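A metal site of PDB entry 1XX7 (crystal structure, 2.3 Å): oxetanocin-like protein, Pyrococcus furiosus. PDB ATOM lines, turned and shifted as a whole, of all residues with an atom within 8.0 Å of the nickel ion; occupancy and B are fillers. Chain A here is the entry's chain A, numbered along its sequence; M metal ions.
The nickel ion is bound by OD1 of Asp 132 (2.0 Å), OD2 of Asp 76 (2.1 Å), NE2 of His 41 (2.2 Å) and NE2 of His 75 (2.3 Å).
The nickel ion has four donor atoms within binding distance.
A ring nitrogen (ND1) of His 75 is in hydrogen-bond range of the backbone carbonyl oxygen of Ala 72 (2.7 Å).
The side-chain hydroxyl (OH) of Tyr 117 sits at hydrogen-bond distance from the side-chain carboxylate (OD2) of Asp 132.
Four residues have an atom within 4 Å of the nickel ion: His 41, His 75, Asp 76 and Asp 132.
The nearest printed residue that does not touch the nickel ion is Tyr 117 (4.3 Å).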
ATOM      1  N   ARG A  24      29.014   7.291 -24.147  1.00  0.00           N
ATOM      2  CA  ARG A  24      27.863   6.452 -24.059  1.00  0.00           C
ATOM      3  C   ARG A  24      28.346   4.986 -24.408  1.00  0.00           C
ATOM      4  O   ARG A  24      28.622   4.643 -25.594  1.00  0.00           O
ATOM      5  CB  ARG A  24      26.833   6.998 -25.037  1.00  0.00           C
ATOM      6  CG  ARG A  24      26.285   8.350 -24.593  1.00  0.00           C
ATOM      7  CD  ARG A  24      25.064   8.157 -23.670  1.00  0.00           C
ATOM      8  NE  ARG A  24      23.899   7.699 -24.456  1.00  0.00           N
ATOM      9  CZ  ARG A  24      22.777   7.157 -23.945  1.00  0.00           C
ATOM     10  NH1 ARG A  24      21.793   6.786 -24.769  1.00  0.00           N
ATOM     11  NH2 ARG A  24      22.646   6.946 -22.638  1.00  0.00           N
ATOM     12  N   VAL A  38      28.078  11.520 -23.143  1.00  0.00           N
ATOM     13  CA  VAL A  38      26.904  11.656 -22.288  1.00  0.00           C
ATOM     14  C   VAL A  38      26.299  13.078 -22.410  1.00  0.00           C
ATOM     15  O   VAL A  38      25.071  13.257 -22.327  1.00  0.00           O
ATOM     16  CB  VAL A  38      27.232  11.296 -20.842  1.00  0.00           C
ATOM     17  CG1 VAL A  38      26.001  11.502 -19.936  1.00  0.00           C
ATOM     18  CG2 VAL A  38      27.693   9.869 -20.762  1.00  0.00           C
ATOM     19  N   HIS A  41      24.323  13.235 -25.726  1.00  0.00           N
ATOM     20  CA  HIS A  41      23.100  12.579 -25.424  1.00  0.00           C
ATOM     21  C   HIS A  41      22.163  13.463 -24.635  1.00  0.00           C
ATOM     22  O   HIS A  41      21.007  13.599 -25.019  1.00  0.00           O
ATOM     23  CB  HIS A  41      23.413  11.336 -24.587  1.00  0.00           C
ATOM     24  CG  HIS A  41      22.238  10.772 -23.902  1.00  0.00           C
ATOM     25  ND1 HIS A  41      21.125  10.328 -24.589  1.00  0.00           N
ATOM     26  CD2 HIS A  41      21.963  10.599 -22.587  1.00  0.00           C
ATOM     27  CE1 HIS A  41      20.230   9.880 -23.727  1.00  0.00           C
ATOM     28  NE2 HIS A  41      20.724  10.018 -22.515  1.00  0.00           N
ATOM     29  N   SER A  42      22.680  14.028 -23.548  1.00  0.00           N
ATOM     30  CA  SER A  42      21.917  14.862 -22.631  1.00  0.00           C
ATOM     31  C   SER A  42      21.429  16.161 -23.221  1.00  0.00           C
ATOM     32  O   SER A  42      20.331  16.643 -22.844  1.00  0.00           O
ATOM     33  CB  SER A  42      22.739  15.185 -21.381  1.00  0.00           C
ATOM     34  OG  SER A  42      23.001  14.037 -20.640  1.00  0.00           O
ATOM     35  N   VAL A  45      18.377  15.064 -25.345  1.00  0.00           N
ATOM     36  CA  VAL A  45      17.296  14.746 -24.381  1.00  0.00           C
ATOM     37  C   VAL A  45      16.558  16.056 -23.927  1.00  0.00           C
ATOM     38  O   VAL A  45      15.315  16.095 -23.909  1.00  0.00           O
ATOM     39  CB  VAL A  45      17.818  13.933 -23.143  1.00  0.00           C
ATOM     40  CG1 VAL A  45      16.747  13.789 -22.066  1.00  0.00           C
ATOM     41  CG2 VAL A  45      18.269  12.561 -23.572  1.00  0.00           C
ATOM     42  N   ALA A  72      15.945  17.091 -17.313  1.00  0.00           N
ATOM     43  CA  ALA A  72      16.632  16.659 -18.496  1.00  0.00           C
ATOM     44  C   ALA A  72      18.155  16.981 -18.451  1.00  0.00           C
ATOM     45  O   ALA A  72      18.976  16.180 -18.852  1.00  0.00           O
ATOM     46  CB  ALA A  72      16.019  17.297 -19.694  1.00  0.00           C
ATOM     47  N   HIS A  75      19.780  14.809 -15.464  1.00  0.00           N
ATOM     48  CA  HIS A  75      19.381  13.416 -15.294  1.00  0.00           C
ATOM     49  C   HIS A  75      20.521  12.371 -15.392  1.00  0.00           C
ATOM     50  O   HIS A  75      20.459  11.332 -14.714  1.00  0.00           O
ATOM     51  CB  HIS A  75      18.215  13.081 -16.185  1.00  0.00           C
ATOM     52  CG  HIS A  75      18.620  12.606 -17.531  1.00  0.00           C
ATOM     53  ND1 HIS A  75      18.996  13.455 -18.539  1.00  0.00           N
ATOM     54  CD2 HIS A  75      18.753  11.351 -18.022  1.00  0.00           C
ATOM     55  CE1 HIS A  75      19.348  12.750 -19.599  1.00  0.00           C
ATOM     56  NE2 HIS A  75      19.188  11.472 -19.317  1.00  0.00           N
ATOM     57  N   ASP A  76      21.566  12.657 -16.175  1.00  0.00           N
ATOM     58  CA  ASP A  76      22.716  11.768 -16.304  1.00  0.00           C
ATOM     59  C   ASP A  76      23.996  12.407 -15.761  1.00  0.00           C
ATOM     60  O   ASP A  76      25.076  11.880 -15.963  1.00  0.00           O
ATOM     61  CB  ASP A  76      22.914  11.364 -17.759  1.00  0.00           C
ATOM     62  CG  ASP A  76      21.974  10.270 -18.204  1.00  0.00           C
ATOM     63  OD1 ASP A  76      21.293   9.687 -17.350  1.00  0.00           O
ATOM     64  OD2 ASP A  76      21.903   9.959 -19.401  1.00  0.00           O
ATOM     65  N   LEU A  77      23.855  13.501 -14.997  1.00  0.00           N
ATOM     66  CA  LEU A  77      25.007  14.205 -14.467  1.00  0.00           C
ATOM     67  C   LEU A  77      25.801  13.387 -13.420  1.00  0.00           C
ATOM     68  O   LEU A  77      27.026  13.575 -13.284  1.00  0.00           O
ATOM     69  CB  LEU A  77      24.534  15.511 -13.860  1.00  0.00           C
ATOM     70  CG  LEU A  77      25.564  16.561 -13.469  1.00  0.00           C
ATOM     71  CD1 LEU A  77      26.692  16.776 -14.556  1.00  0.00           C
ATOM     72  CD2 LEU A  77      24.789  17.857 -13.191  1.00  0.00           C
ATOM     73  N   GLU A  79      26.624  10.476 -13.859  1.00  0.00           N
ATOM     74  CA  GLU A  79      27.547   9.702 -14.671  1.00  0.00           C
ATOM     75  C   GLU A  79      28.912  10.377 -14.828  1.00  0.00           C
ATOM     76  O   GLU A  79      29.876   9.714 -15.167  1.00  0.00           O
ATOM     77  CB  GLU A  79      26.919   9.357 -16.040  1.00  0.00           C
ATOM     78  CG  GLU A  79      25.630   8.589 -15.852  1.00  0.00           C
ATOM     79  CD  GLU A  79      25.028   7.995 -17.119  1.00  0.00           C
ATOM     80  OE1 GLU A  79      25.352   8.407 -18.262  1.00  0.00           O
ATOM     81  OE2 GLU A  79      24.171   7.125 -16.941  1.00  0.00           O
ATOM     82  N   ASP A  84      28.879   5.959 -17.556  1.00  0.00           N
ATOM     83  CA  ASP A  84      27.676   5.429 -18.127  1.00  0.00           C
ATOM     84  C   ASP A  84      27.793   3.879 -18.095  1.00  0.00           C
ATOM     85  O   ASP A  84      28.304   3.267 -19.011  1.00  0.00           O
ATOM     86  CB  ASP A  84      27.531   5.955 -19.564  1.00  0.00           C
ATOM     87  CG  ASP A  84      26.259   5.483 -20.223  1.00  0.00           C
ATOM     88  OD1 ASP A  84      25.297   5.172 -19.507  1.00  0.00           O
ATOM     89  OD2 ASP A  84      26.232   5.391 -21.457  1.00  0.00           O
ATOM     90  N   GLU A  99      24.353   6.549  -8.888  1.00  0.00           N
ATOM     91  CA  GLU A  99      24.192   7.936  -9.452  1.00  0.00           C
ATOM     92  C   GLU A  99      23.488   8.867  -8.463  1.00  0.00           C
ATOM     93  O   GLU A  99      23.890  10.027  -8.329  1.00  0.00           O
ATOM     94  CB  GLU A  99      23.403   7.941 -10.773  1.00  0.00           C
ATOM     95  CG  GLU A  99      24.110   7.327 -11.987  1.00  0.00           C
ATOM     96  CD  GLU A  99      23.310   7.524 -13.317  1.00  0.00           C
ATOM     97  OE1 GLU A  99      22.649   8.566 -13.517  1.00  0.00           O
ATOM     98  OE2 GLU A  99      23.370   6.620 -14.184  1.00  0.00           O
ATOM     99  N   TYR A 117      13.008  11.654 -12.095  1.00  0.00           N
ATOM    100  CA  TYR A 117      13.470  11.042 -13.340  1.00  0.00           C
ATOM    101  C   TYR A 117      13.509   9.512 -13.124  1.00  0.00           C
ATOM    102  O   TYR A 117      12.907   8.740 -13.926  1.00  0.00           O
ATOM    103  CB  TYR A 117      14.842  11.578 -13.807  1.00  0.00           C
ATOM    104  CG  TYR A 117      15.344  10.798 -15.005  1.00  0.00           C
ATOM    105  CD1 TYR A 117      14.758  10.969 -16.228  1.00  0.00           C
ATOM    106  CD2 TYR A 117      16.341   9.825 -14.879  1.00  0.00           C
ATOM    107  CE1 TYR A 117      15.136  10.273 -17.302  1.00  0.00           C
ATOM    108  CE2 TYR A 117      16.742   9.083 -16.004  1.00  0.00           C
ATOM    109  CZ  TYR A 117      16.112   9.317 -17.193  1.00  0.00           C
ATOM    110  OH  TYR A 117      16.431   8.659 -18.351  1.00  0.00           O
ATOM    111  N   VAL A 128      10.632  13.117 -19.376  1.00  0.00           N
ATOM    112  CA  VAL A 128      12.066  13.068 -19.587  1.00  0.00           C
ATOM    113  C   VAL A 128      12.537  11.635 -19.837  1.00  0.00           C
ATOM    114  O   VAL A 128      13.440  11.423 -20.631  1.00  0.00           O
ATOM    115  CB  VAL A 128      12.851  13.719 -18.428  1.00  0.00           C
ATOM    116  CG1 VAL A 128      14.332  13.672 -18.730  1.00  0.00           C
ATOM    117  CG2 VAL A 128      12.429  15.173 -18.237  1.00  0.00           C
ATOM    118  N   LYS A 129      11.906  10.652 -19.186  1.00  0.00           N
ATOM    119  CA  LYS A 129      12.134   9.251 -19.522  1.00  0.00           C
ATOM    120  C   LYS A 129      11.802   8.896 -20.981  1.00  0.00           C
ATOM    121  O   LYS A 129      12.531   8.144 -21.674  1.00  0.00           O
ATOM    122  CB  LYS A 129      11.352   8.322 -18.554  1.00  0.00           C
ATOM    123  CG  LYS A 129      11.810   6.836 -18.584  1.00  0.00           C
ATOM    124  CD  LYS A 129      13.200   6.581 -17.943  1.00  0.00           C
ATOM    125  CE  LYS A 129      13.069   6.430 -16.410  1.00  0.00           C
ATOM    126  NZ  LYS A 129      14.335   6.255 -15.614  1.00  0.00           N
ATOM    127  N   ALA A 131      11.829  11.123 -23.454  1.00  0.00           N
ATOM    128  CA  ALA A 131      12.812  11.848 -24.283  1.00  0.00           C
ATOM    129  C   ALA A 131      14.145  11.104 -24.339  1.00  0.00           C
ATOM    130  O   ALA A 131      14.796  11.042 -25.345  1.00  0.00           O
ATOM    131  CB  ALA A 131      13.030  13.267 -23.713  1.00  0.00           C
ATOM    132  N   ASP A 132      14.553  10.578 -23.201  1.00  0.00           N
ATOM    133  CA  ASP A 132      15.787   9.844 -23.067  1.00  0.00           C
ATOM    134  C   ASP A 132      15.855   8.584 -23.964  1.00  0.00           C
ATOM    135  O   ASP A 132      16.847   8.324 -24.674  1.00  0.00           O
ATOM    136  CB  ASP A 132      15.938   9.494 -21.612  1.00  0.00           C
ATOM    137  CG  ASP A 132      17.250   8.835 -21.325  1.00  0.00           C
ATOM    138  OD1 ASP A 132      18.275   9.491 -21.403  1.00  0.00           O
ATOM    139  OD2 ASP A 132      17.264   7.633 -21.051  1.00  0.00           O
ATOM    140  N   LYS A 133      14.761   7.820 -23.918  1.00  0.00           N
ATOM    141  CA  LYS A 133      14.593   6.642 -24.745  1.00  0.00           C
ATOM    142  C   LYS A 133      14.483   6.962 -26.196  1.00  0.00           C
ATOM    143  O   LYS A 133      15.008   6.247 -27.037  1.00  0.00           O
ATOM    144  CB  LYS A 133      13.388   5.840 -24.247  1.00  0.00           C
ATOM    145  CG  LYS A 133      13.700   5.160 -22.904  1.00  0.00           C
ATOM    146  CD  LYS A 133      12.455   4.724 -22.157  1.00  0.00           C
ATOM    147  CE  LYS A 133      12.811   3.995 -20.859  1.00  0.00           C
ATOM    148  NZ  LYS A 133      13.979   3.054 -21.073  1.00  0.00           N
ATOM    149  N   ASP A 135      15.863   9.682 -27.728  1.00  0.00           N
ATOM    150  CA  ASP A 135      17.186  10.041 -28.163  1.00  0.00           C
ATOM    151  C   ASP A 135      18.003   8.761 -28.524  1.00  0.00           C
ATOM    152  O   ASP A 135      18.616   8.695 -29.582  1.00  0.00           O
ATOM    153  CB  ASP A 135      17.929  10.804 -27.089  1.00  0.00           C
ATOM    154  CG  ASP A 135      19.383  11.001 -27.430  1.00  0.00           C
ATOM    155  OD1 ASP A 135      19.698  11.752 -28.396  1.00  0.00           O
ATOM    156  OD2 ASP A 135      20.207  10.376 -26.757  1.00  0.00           O
ATOM    157  N   MET A 136      17.960   7.759 -27.645  1.00  0.00           N
ATOM    158  CA  MET A 136      18.653   6.471 -27.822  1.00  0.00           C
ATOM    159  C   MET A 136      18.232   5.685 -29.051  1.00  0.00           C
ATOM    160  O   MET A 136      19.076   5.186 -29.763  1.00  0.00           O
ATOM    161  CB  MET A 136      18.483   5.588 -26.594  1.00  0.00           C
ATOM    162  CG  MET A 136      19.467   4.432 -26.592  1.00  0.00           C
ATOM    163  SD  MET A 136      19.388   3.335 -25.119  1.00  0.00           S
ATOM    164  CE  MET A 136      17.883   2.448 -25.654  1.00  0.00           C
HETATM  165 NI    NI M   1      20.044   9.619 -20.422  1.00  0.00          NI
